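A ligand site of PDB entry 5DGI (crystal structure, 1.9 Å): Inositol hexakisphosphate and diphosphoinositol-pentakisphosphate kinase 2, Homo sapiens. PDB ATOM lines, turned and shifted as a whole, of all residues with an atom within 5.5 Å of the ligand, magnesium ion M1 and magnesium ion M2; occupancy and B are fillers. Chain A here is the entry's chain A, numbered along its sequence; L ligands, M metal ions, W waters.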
ATOM      1  N   ARG A  98       9.413 -15.753  17.155  1.00  0.00           N
ATOM      2  CA  ARG A  98      10.211 -15.014  18.148  1.00  0.00           C
ATOM      3  C   ARG A  98       9.779 -13.559  18.296  1.00  0.00           C
ATOM      4  O   ARG A  98       9.832 -13.006  19.396  1.00  0.00           O
ATOM      5  CB  ARG A  98      11.705 -15.082  17.830  1.00  0.00           C
ATOM      6  CG  ARG A  98      12.290 -16.484  17.875  1.00  0.00           C
ATOM      7  CD  ARG A  98      13.810 -16.461  17.795  1.00  0.00           C
ATOM      8  NE  ARG A  98      14.350 -17.764  17.392  1.00  0.00           N
ATOM      9  CZ  ARG A  98      14.564 -18.786  18.213  1.00  0.00           C
ATOM     10  NH1 ARG A  98      14.307 -18.679  19.507  1.00  0.00           N
ATOM     11  NH2 ARG A  98      15.040 -19.928  17.737  1.00  0.00           N
ATOM     12  N   TYR A 102       8.682 -11.991  21.901  1.00  0.00           N
ATOM     13  CA  TYR A 102       9.317 -10.787  22.450  1.00  0.00           C
ATOM     14  C   TYR A 102       8.334  -9.643  22.700  1.00  0.00           C
ATOM     15  O   TYR A 102       8.475  -8.904  23.685  1.00  0.00           O
ATOM     16  CB  TYR A 102      10.468 -10.339  21.541  1.00  0.00           C
ATOM     17  CG  TYR A 102      11.799 -10.972  21.898  1.00  0.00           C
ATOM     18  CD1 TYR A 102      11.863 -12.229  22.522  1.00  0.00           C
ATOM     19  CD2 TYR A 102      12.993 -10.326  21.598  1.00  0.00           C
ATOM     20  CE1 TYR A 102      13.076 -12.803  22.853  1.00  0.00           C
ATOM     21  CE2 TYR A 102      14.221 -10.903  21.930  1.00  0.00           C
ATOM     22  CZ  TYR A 102      14.254 -12.132  22.549  1.00  0.00           C
ATOM     23  OH  TYR A 102      15.465 -12.690  22.864  1.00  0.00           O
ATOM     24  N   PRO A 113      16.694  -8.890  26.398  1.00  0.00           N
ATOM     25  CA  PRO A 113      17.751  -8.144  25.727  1.00  0.00           C
ATOM     26  C   PRO A 113      17.174  -7.056  24.822  1.00  0.00           C
ATOM     27  O   PRO A 113      16.133  -7.274  24.190  1.00  0.00           O
ATOM     28  CB  PRO A 113      18.447  -9.205  24.872  1.00  0.00           C
ATOM     29  CG  PRO A 113      18.111 -10.508  25.517  1.00  0.00           C
ATOM     30  CD  PRO A 113      16.722 -10.322  26.046  1.00  0.00           C
ATOM     31  N   VAL A 149      23.662 -10.953  19.075  1.00  0.00           N
ATOM     32  CA  VAL A 149      23.055 -12.247  18.760  1.00  0.00           C
ATOM     33  C   VAL A 149      22.074 -12.081  17.598  1.00  0.00           C
ATOM     34  O   VAL A 149      21.357 -11.090  17.521  1.00  0.00           O
ATOM     35  CB  VAL A 149      22.334 -12.875  19.984  1.00  0.00           C
ATOM     36  CG1 VAL A 149      21.785 -14.259  19.648  1.00  0.00           C
ATOM     37  CG2 VAL A 149      23.263 -12.953  21.192  1.00  0.00           C
ATOM     38  N   LYS A 151      19.015 -14.141  15.651  1.00  0.00           N
ATOM     39  CA  LYS A 151      18.081 -15.264  15.748  1.00  0.00           C
ATOM     40  C   LYS A 151      17.095 -15.280  14.575  1.00  0.00           C
ATOM     41  O   LYS A 151      16.499 -14.251  14.271  1.00  0.00           O
ATOM     42  CB  LYS A 151      17.298 -15.219  17.063  1.00  0.00           C
ATOM     43  CG  LYS A 151      18.145 -15.059  18.310  1.00  0.00           C
ATOM     44  CD  LYS A 151      17.317 -15.238  19.579  1.00  0.00           C
ATOM     45  CE  LYS A 151      18.178 -14.979  20.805  1.00  0.00           C
ATOM     46  NZ  LYS A 151      17.435 -15.045  22.092  1.00  0.00           N
ATOM     47  N   ALA A 155      10.810 -19.462  15.708  1.00  0.00           N
ATOM     48  CA  ALA A 155      11.287 -19.991  16.980  1.00  0.00           C
ATOM     49  C   ALA A 155      11.600 -21.489  16.875  1.00  0.00           C
ATOM     50  O   ALA A 155      12.216 -22.066  17.766  1.00  0.00           O
ATOM     51  CB  ALA A 155      10.262 -19.724  18.070  1.00  0.00           C
ATOM     52  N   ASP A 157      13.405 -22.557  14.433  1.00  0.00           N
ATOM     53  CA  ASP A 157      14.718 -22.556  13.781  1.00  0.00           C
ATOM     54  C   ASP A 157      15.767 -22.187  14.825  1.00  0.00           C
ATOM     55  O   ASP A 157      15.785 -21.060  15.315  1.00  0.00           O
ATOM     56  CB  ASP A 157      14.730 -21.568  12.603  1.00  0.00           C
ATOM     57  CG  ASP A 157      16.022 -21.636  11.788  1.00  0.00           C
ATOM     58  OD1 ASP A 157      17.084 -22.043  12.314  1.00  0.00           O
ATOM     59  OD2 ASP A 157      15.971 -21.256  10.599  1.00  0.00           O
ATOM     60  N   HIS A 158      16.623 -23.161  15.158  1.00  0.00           N
ATOM     61  CA  HIS A 158      17.589 -23.019  16.250  1.00  0.00           C
ATOM     62  C   HIS A 158      18.993 -22.638  15.791  1.00  0.00           C
ATOM     63  O   HIS A 158      19.964 -22.692  16.553  1.00  0.00           O
ATOM     64  CB  HIS A 158      17.571 -24.305  17.090  1.00  0.00           C
ATOM     65  CG  HIS A 158      16.206 -24.649  17.602  1.00  0.00           C
ATOM     66  ND1 HIS A 158      15.596 -23.942  18.609  1.00  0.00           N
ATOM     67  CD2 HIS A 158      15.307 -25.583  17.194  1.00  0.00           C
ATOM     68  CE1 HIS A 158      14.400 -24.442  18.835  1.00  0.00           C
ATOM     69  NE2 HIS A 158      14.197 -25.443  17.985  1.00  0.00           N
ATOM     70  N   VAL A 160      20.878 -20.103  15.698  1.00  0.00           N
ATOM     71  CA  VAL A 160      21.154 -18.816  16.326  1.00  0.00           C
ATOM     72  C   VAL A 160      22.663 -18.546  16.243  1.00  0.00           C
ATOM     73  O   VAL A 160      23.465 -19.415  16.606  1.00  0.00           O
ATOM     74  CB  VAL A 160      20.679 -18.823  17.804  1.00  0.00           C
ATOM     75  CG1 VAL A 160      21.175 -17.583  18.539  1.00  0.00           C
ATOM     76  CG2 VAL A 160      19.162 -18.939  17.903  1.00  0.00           C
ATOM     77  N   ILE A 162      26.077 -15.955  17.065  1.00  0.00           N
ATOM     78  CA  ILE A 162      26.667 -14.897  17.889  1.00  0.00           C
ATOM     79  C   ILE A 162      27.889 -14.340  17.156  1.00  0.00           C
ATOM     80  O   ILE A 162      28.680 -15.098  16.623  1.00  0.00           O
ATOM     81  CB  ILE A 162      27.027 -15.414  19.304  1.00  0.00           C
ATOM     82  CG1 ILE A 162      25.773 -16.018  19.965  1.00  0.00           C
ATOM     83  CG2 ILE A 162      27.646 -14.309  20.146  1.00  0.00           C
ATOM     84  CD1 ILE A 162      25.906 -16.374  21.423  1.00  0.00           C
ATOM     85  N   LEU A 175      25.184 -21.723  16.581  1.00  0.00           N
ATOM     86  CA  LEU A 175      24.456 -22.680  17.418  1.00  0.00           C
ATOM     87  C   LEU A 175      23.462 -23.436  16.565  1.00  0.00           C
ATOM     88  O   LEU A 175      23.042 -22.962  15.520  1.00  0.00           O
ATOM     89  CB  LEU A 175      23.727 -21.936  18.548  1.00  0.00           C
ATOM     90  CG  LEU A 175      24.546 -21.323  19.691  1.00  0.00           C
ATOM     91  CD1 LEU A 175      25.605 -20.316  19.228  1.00  0.00           C
ATOM     92  CD2 LEU A 175      23.599 -20.654  20.669  1.00  0.00           C
ATOM     93  N   GLU A 201      19.924  -8.798  18.718  1.00  0.00           N
ATOM     94  CA  GLU A 201      19.852  -8.394  20.118  1.00  0.00           C
ATOM     95  C   GLU A 201      21.220  -8.302  20.784  1.00  0.00           C
ATOM     96  O   GLU A 201      22.173  -8.960  20.352  1.00  0.00           O
ATOM     97  CB  GLU A 201      18.904  -9.312  20.907  1.00  0.00           C
ATOM     98  CG  GLU A 201      19.345 -10.753  21.017  1.00  0.00           C
ATOM     99  CD  GLU A 201      18.273 -11.653  21.611  1.00  0.00           C
ATOM    100  OE1 GLU A 201      18.546 -12.253  22.675  1.00  0.00           O
ATOM    101  OE2 GLU A 201      17.173 -11.778  21.031  1.00  0.00           O
ATOM    102  N   GLU A 202      21.276  -7.490  21.836  1.00  0.00           N
ATOM    103  CA  GLU A 202      22.497  -7.349  22.635  1.00  0.00           C
ATOM    104  C   GLU A 202      22.862  -8.663  23.331  1.00  0.00           C
ATOM    105  O   GLU A 202      21.975  -9.402  23.806  1.00  0.00           O
ATOM    106  CB  GLU A 202      22.379  -6.210  23.655  1.00  0.00           C
ATOM    107  CG  GLU A 202      21.164  -6.308  24.561  1.00  0.00           C
ATOM    108  CD  GLU A 202      21.260  -5.456  25.821  1.00  0.00           C
ATOM    109  OE1 GLU A 202      22.361  -4.945  26.141  1.00  0.00           O
ATOM    110  OE2 GLU A 202      20.229  -5.326  26.507  1.00  0.00           O
ATOM    111  N   PHE A 203      24.157  -8.945  23.358  1.00  0.00           N
ATOM    112  CA  PHE A 203      24.681 -10.119  24.023  1.00  0.00           C
ATOM    113  C   PHE A 203      24.734  -9.848  25.514  1.00  0.00           C
ATOM    114  O   PHE A 203      25.357  -8.870  25.956  1.00  0.00           O
ATOM    115  CB  PHE A 203      26.080 -10.444  23.487  1.00  0.00           C
ATOM    116  CG  PHE A 203      26.724 -11.652  24.113  1.00  0.00           C
ATOM    117  CD1 PHE A 203      26.477 -12.929  23.596  1.00  0.00           C
ATOM    118  CD2 PHE A 203      27.564 -11.527  25.205  1.00  0.00           C
ATOM    119  CE1 PHE A 203      27.070 -14.049  24.167  1.00  0.00           C
ATOM    120  CE2 PHE A 203      28.149 -12.638  25.794  1.00  0.00           C
ATOM    121  CZ  PHE A 203      27.907 -13.896  25.270  1.00  0.00           C
ATOM    122  N   MET A 204      24.055 -10.687  26.291  1.00  0.00           N
ATOM    123  CA  MET A 204      24.047 -10.563  27.748  1.00  0.00           C
ATOM    124  C   MET A 204      25.119 -11.470  28.338  1.00  0.00           C
ATOM    125  O   MET A 204      25.074 -12.684  28.135  1.00  0.00           O
ATOM    126  CB  MET A 204      22.665 -10.936  28.313  1.00  0.00           C
ATOM    127  CG  MET A 204      21.469 -10.337  27.575  1.00  0.00           C
ATOM    128  SD  MET A 204      21.545  -8.542  27.344  1.00  0.00           S
ATOM    129  CE  MET A 204      21.545  -7.967  29.032  1.00  0.00           C
ATOM    130  N   PRO A 205      26.090 -10.888  29.068  1.00  0.00           N
ATOM    131  CA  PRO A 205      27.203 -11.684  29.577  1.00  0.00           C
ATOM    132  C   PRO A 205      26.840 -12.465  30.839  1.00  0.00           C
ATOM    133  O   PRO A 205      26.594 -11.873  31.898  1.00  0.00           O
ATOM    134  CB  PRO A 205      28.286 -10.640  29.849  1.00  0.00           C
ATOM    135  CG  PRO A 205      27.541  -9.373  30.121  1.00  0.00           C
ATOM    136  CD  PRO A 205      26.221  -9.463  29.409  1.00  0.00           C
ATOM    137  N   ASP A 210      23.199 -21.079  30.985  1.00  0.00           N
ATOM    138  CA  ASP A 210      21.816 -20.643  30.810  1.00  0.00           C
ATOM    139  C   ASP A 210      20.992 -21.200  31.963  1.00  0.00           C
ATOM    140  O   ASP A 210      21.248 -22.317  32.423  1.00  0.00           O
ATOM    141  CB  ASP A 210      21.200 -21.238  29.535  1.00  0.00           C
ATOM    142  CG  ASP A 210      21.952 -20.877  28.284  1.00  0.00           C
ATOM    143  OD1 ASP A 210      22.560 -19.783  28.231  1.00  0.00           O
ATOM    144  OD2 ASP A 210      21.925 -21.684  27.330  1.00  0.00           O
ATOM    145  N   LYS A 212      17.439 -22.651  32.821  1.00  0.00           N
ATOM    146  CA  LYS A 212      16.258 -23.232  32.184  1.00  0.00           C
ATOM    147  C   LYS A 212      15.134 -23.334  33.201  1.00  0.00           C
ATOM    148  O   LYS A 212      15.295 -24.002  34.233  1.00  0.00           O
ATOM    149  CB  LYS A 212      16.568 -24.639  31.634  1.00  0.00           C
ATOM    150  CG  LYS A 212      17.827 -24.737  30.786  1.00  0.00           C
ATOM    151  CD  LYS A 212      17.625 -24.031  29.472  1.00  0.00           C
ATOM    152  CE  LYS A 212      18.782 -24.267  28.516  1.00  0.00           C
ATOM    153  NZ  LYS A 212      18.407 -23.764  27.162  1.00  0.00           N
ATOM    154  N   SER A 228      26.180 -22.809  28.463  1.00  0.00           N
ATOM    155  CA  SER A 228      25.685 -22.095  27.292  1.00  0.00           C
ATOM    156  C   SER A 228      26.303 -22.681  26.037  1.00  0.00           C
ATOM    157  O   SER A 228      27.521 -22.842  25.970  1.00  0.00           O
ATOM    158  CB  SER A 228      26.039 -20.604  27.370  1.00  0.00           C
ATOM    159  OG  SER A 228      25.864 -19.999  26.094  1.00  0.00           O
ATOM    160  N   PRO A 229      25.474 -23.018  25.025  1.00  0.00           N
ATOM    161  CA  PRO A 229      26.009 -23.583  23.775  1.00  0.00           C
ATOM    162  C   PRO A 229      27.009 -22.646  23.102  1.00  0.00           C
ATOM    163  O   PRO A 229      27.868 -23.105  22.347  1.00  0.00           O
ATOM    164  CB  PRO A 229      24.755 -23.740  22.899  1.00  0.00           C
ATOM    165  CG  PRO A 229      23.623 -23.831  23.863  1.00  0.00           C
ATOM    166  CD  PRO A 229      23.996 -22.936  25.010  1.00  0.00           C
ATOM    167  N   ALA A 230      26.908 -21.355  23.402  1.00  0.00           N
ATOM    168  CA  ALA A 230      27.776 -20.344  22.827  1.00  0.00           C
ATOM    169  C   ALA A 230      29.230 -20.371  23.321  1.00  0.00           C
ATOM    170  O   ALA A 230      30.113 -19.815  22.666  1.00  0.00           O
ATOM    171  CB  ALA A 230      27.179 -18.962  23.055  1.00  0.00           C
ATOM    172  N   ASP A 273      13.904 -19.684  28.937  1.00  0.00           N
ATOM    173  CA  ASP A 273      15.296 -19.471  29.338  1.00  0.00           C
ATOM    174  C   ASP A 273      15.522 -18.129  29.988  1.00  0.00           C
ATOM    175  O   ASP A 273      14.986 -17.105  29.554  1.00  0.00           O
ATOM    176  CB  ASP A 273      16.240 -19.564  28.146  1.00  0.00           C
ATOM    177  CG  ASP A 273      16.197 -20.903  27.472  1.00  0.00           C
ATOM    178  OD1 ASP A 273      16.040 -21.935  28.134  1.00  0.00           O
ATOM    179  OD2 ASP A 273      16.339 -20.889  26.262  1.00  0.00           O
ATOM    180  N   LEU A 275      18.721 -15.540  31.291  1.00  0.00           N
ATOM    181  CA  LEU A 275      20.118 -15.178  31.283  1.00  0.00           C
ATOM    182  C   LEU A 275      20.377 -14.321  32.510  1.00  0.00           C
ATOM    183  O   LEU A 275      19.836 -13.224  32.633  1.00  0.00           O
ATOM    184  CB  LEU A 275      20.491 -14.435  29.991  1.00  0.00           C
ATOM    185  CG  LEU A 275      20.137 -15.154  28.671  1.00  0.00           C
ATOM    186  CD1 LEU A 275      20.496 -14.286  27.478  1.00  0.00           C
ATOM    187  CD2 LEU A 275      20.813 -16.517  28.575  1.00  0.00           C
ATOM    188  N   CYS A 284      15.137 -14.828  27.234  1.00  0.00           N
ATOM    189  CA  CYS A 284      15.611 -14.780  25.846  1.00  0.00           C
ATOM    190  C   CYS A 284      14.881 -15.751  24.896  1.00  0.00           C
ATOM    191  O   CYS A 284      15.143 -15.748  23.699  1.00  0.00           O
ATOM    192  CB  CYS A 284      17.141 -14.974  25.763  1.00  0.00           C
ATOM    193  SG  CYS A 284      17.718 -16.652  26.135  1.00  0.00           S
ATOM    194  N   ASP A 285      13.964 -16.541  25.440  1.00  0.00           N
ATOM    195  CA  ASP A 285      13.339 -17.656  24.719  1.00  0.00           C
ATOM    196  C   ASP A 285      12.192 -18.192  25.559  1.00  0.00           C
ATOM    197  O   ASP A 285      12.365 -18.421  26.749  1.00  0.00           O
ATOM    198  CB  ASP A 285      14.400 -18.760  24.497  1.00  0.00           C
ATOM    199  CG  ASP A 285      13.930 -19.906  23.588  1.00  0.00           C
ATOM    200  OD1 ASP A 285      13.037 -19.747  22.724  1.00  0.00           O
ATOM    201  OD2 ASP A 285      14.498 -21.006  23.722  1.00  0.00           O
ATOM    202  N   VAL A 286      11.025 -18.338  24.949  1.00  0.00           N
ATOM    203  CA  VAL A 286       9.876 -18.976  25.588  1.00  0.00           C
ATOM    204  C   VAL A 286       9.421 -20.116  24.676  1.00  0.00           C
ATOM    205  O   VAL A 286       9.086 -19.892  23.518  1.00  0.00           O
ATOM    206  CB  VAL A 286       8.704 -17.988  25.846  1.00  0.00           C
ATOM    207  CG1 VAL A 286       7.496 -18.713  26.462  1.00  0.00           C
ATOM    208  CG2 VAL A 286       9.144 -16.851  26.744  1.00  0.00           C
ATOM    209  N   ASN A 287       9.412 -21.330  25.234  1.00  0.00           N
ATOM    210  CA  ASN A 287       9.225 -22.537  24.430  1.00  0.00           C
ATOM    211  C   ASN A 287       7.878 -23.206  24.531  1.00  0.00           C
ATOM    212  O   ASN A 287       7.568 -24.102  23.734  1.00  0.00           O
ATOM    213  CB  ASN A 287      10.337 -23.537  24.759  1.00  0.00           C
ATOM    214  CG  ASN A 287      11.690 -23.022  24.348  1.00  0.00           C
ATOM    215  OD1 ASN A 287      11.808 -22.458  23.277  1.00  0.00           O
ATOM    216  ND2 ASN A 287      12.694 -23.162  25.211  1.00  0.00           N
HETATM  217  P1  LIG L   1      16.460 -21.470  20.959  1.00  0.00           P
HETATM  218  O1  LIG L   1      15.021 -21.135  20.706  1.00  0.00           O
HETATM  219  O2  LIG L   1      17.138 -22.062  19.745  1.00  0.00           O
HETATM  220  O3  LIG L   1      16.752 -22.231  22.197  1.00  0.00           O
HETATM  221  P2  LIG L   1      17.576 -19.090  22.342  1.00  0.00           P
HETATM  222  O4  LIG L   1      17.007 -17.704  22.171  1.00  0.00           O
HETATM  223  O5  LIG L   1      17.457 -19.773  23.668  1.00  0.00           O
HETATM  224  O6  LIG L   1      17.119 -19.985  21.078  1.00  0.00           O
HETATM  225  O7  LIG L   1      19.156 -18.951  22.077  1.00  0.00           O
HETATM  226  C1  LIG L   1      19.999 -20.093  22.207  1.00  0.00           C
HETATM  227  C2  LIG L   1      21.120 -19.819  23.201  1.00  0.00           C
HETATM  228  O8  LIG L   1      21.902 -18.705  22.759  1.00  0.00           O
HETATM  229  C3  LIG L   1      20.650 -19.457  24.605  1.00  0.00           C
HETATM  230  O9  LIG L   1      20.401 -20.604  25.412  1.00  0.00           O
HETATM  231  C4  LIG L   1      21.812 -18.645  25.122  1.00  0.00           C
HETATM  232  O10 LIG L   1      22.878 -19.478  25.601  1.00  0.00           O
HETATM  233  C5  LIG L   1      22.327 -17.939  23.871  1.00  0.00           C
HETATM  234  N1  LIG L   1      21.697 -16.602  23.785  1.00  0.00           N
HETATM  235  C6  LIG L   1      20.511 -16.309  23.194  1.00  0.00           C
HETATM  236  N2  LIG L   1      20.246 -14.983  23.291  1.00  0.00           N
HETATM  237  C7  LIG L   1      21.284 -14.427  23.948  1.00  0.00           C
HETATM  238  C8  LIG L   1      21.654 -13.065  24.394  1.00  0.00           C
HETATM  239  N3  LIG L   1      20.838 -12.032  24.136  1.00  0.00           N
HETATM  240  N4  LIG L   1      22.826 -12.909  25.053  1.00  0.00           N
HETATM  241  C9  LIG L   1      23.647 -13.948  25.323  1.00  0.00           C
HETATM  242  N5  LIG L   1      23.378 -15.205  24.938  1.00  0.00           N
HETATM  243  C10 LIG L   1      22.233 -15.495  24.269  1.00  0.00           C
HETATM  244 MG    MG M   1      13.422 -21.793  21.990  1.00  0.00          MG
HETATM  245 MG    MG M   2      16.505 -21.616  24.247  1.00  0.00          MG
HETATM  246  O   HOH W   1      25.379 -16.805  26.393  1.00  0.00           O
HETATM  247  O   HOH W   2      14.100 -16.423  21.241  1.00  0.00           O
HETATM  248  O   HOH W   3      14.106 -23.863  22.020  1.00  0.00           O
HETATM  249  O   HOH W   4      18.450 -22.420  24.806  1.00  0.00           O
HETATM  250  O   HOH W   5      15.734 -23.548  24.866  1.00  0.00           O
HETATM  251  O   HOH W   6      19.753 -22.273  19.352  1.00  0.00           O
HETATM  252  O   HOH W   7      11.995 -21.790  20.366  1.00  0.00           O
HETATM  253  O   HOH W   8      19.129 -24.255  23.053  1.00  0.00           O
HETATM  254  O   HOH W   9      16.557 -25.257  22.373  1.00  0.00           O
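The side-chain carboxylate (OD1) of Asp 210 lies within hydrogen-bond range of an oxygen (O10) of the ligand (2.7 Å).
O2 of the ligand lies within hydrogen-bond range of ND1 of His 158, at 2.7 Å.
The backbone carbonyl oxygen of Glu 202 lies within hydrogen-bond range of a nitrogen (N3) of the ligand, at 2.9 Å.
A nitrogen (N3) of the ligand lies within hydrogen-bond range of the side-chain carboxylate (OE1) of Glu 201 (2.7 Å).
N4 of the ligand is in hydrogen-bond range of N of Met 204 (2.8 Å).
The side-chain amino group (NZ) of Lys 151 lies within salt-bridge range of an oxygen (O4) of the ligand.
The side-chain hydroxyl of Ser 228 lies within hydrogen-bond range of an oxygen (O10) of the ligand (3.1 Å).
NH2 of Arg 98 is in salt-bridge range of O2 of the ligand, 3.6 Å away.
The side-chain amino group (NZ) of Lys 151 lies within hydrogen-bond range of the side-chain hydroxyl (OH) of Tyr 102 (3.2 Å).
The side-chain carboxylate (OE2) of Glu 201 sits at hydrogen-bond distance from the side-chain hydroxyl (OH) of Tyr 102, 2.7 Å away.
O of Asp 273 lies within hydrogen-bond range of N of Cys 284, 3.3 Å away.
O of Cys 284 lies within hydrogen-bond range of OH of Tyr 102, 3.2 Å away.
The side-chain amino group of Lys 151 lies within salt-bridge range of the side-chain carboxylate of Glu 201.
The guanidinium group of Arg 98 sits close to the side-chain carboxylate of Asp 285 (3.6 Å).
The side-chain carboxylate (OD1) of Asp 273 is in salt-bridge range of the side-chain amino group (NZ) of Lys 212.
N of Ala 230 sits close to OG of Ser 228 (3.2 Å).
O4 of the ligand lies close to O of Cys 284.
CG of Pro 113 touches N3 of the ligand, 3.4 Å away.
CG2 of Val 149 touches C8 of the ligand, at 3.6 Å.
CG2 of Val 160 touches O6 of the ligand, at 3.9 Å.
Leu 175 touches the ligand (CD2 to O8, 3.3 Å).
CD1 of Phe 203 touches C9 of the ligand (3.5 Å).
CD of Pro 229 touches O10 of the ligand, at 3.7 Å.
CD1 of Leu 275 touches C8 of the ligand, at 3.5 Å.
18 residues have an atom within 4 Å of the ligand: Arg 98, Pro 113, Val 149, Lys 151, His 158, Val 160, Leu 175, Glu 201, Glu 202, Phe 203, Met 204, Asp 210, Ser 228, Pro 229, Asp 273, Leu 275, Cys 284 and Asp 285.
Within 4 Å of magnesium ion M1: Asp 285 and Asn 287.
The nearest printed residue that does not touch magnesium ion M1 is Arg 98 (4.1 Å).
Two residues have an atom within 4 Å of magnesium ion M2: Asp 273 and Asp 285.
Magnesium ion M1 is bound by O1 of the ligand, water W7, OD1 of Asn 287, water W3, OD2 of Asp 285 and OD1 of Asp 285.
Magnesium ion M2 is bound by OD2 of Asp 273 (2.1 Å), O5 of the ligand (2.2 Å), O3 of the ligand (2.2 Å), OD2 of Asp 285 (2.2 Å), water W5 (2.2 Å) and water W4 (2.2 Å).
Water W4 bridges NZ of Lys 212 (2.7 Å) and O9 of the ligand (2.7 Å).
Water W6 bridges O2 of the ligand (2.7 Å) and O of His 158 (2.8 Å).
Water W1 bridges N5 of the ligand (2.9 Å) and OG of Ser 228 (3.2 Å).
Water W2 lies within hydrogen-bond range of the backbone carbonyl oxygen of Cys 284 (2.8 Å), the guanidinium group of Arg 98 (2.9 Å) and an oxygen (O4) of the ligand (3.3 Å).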
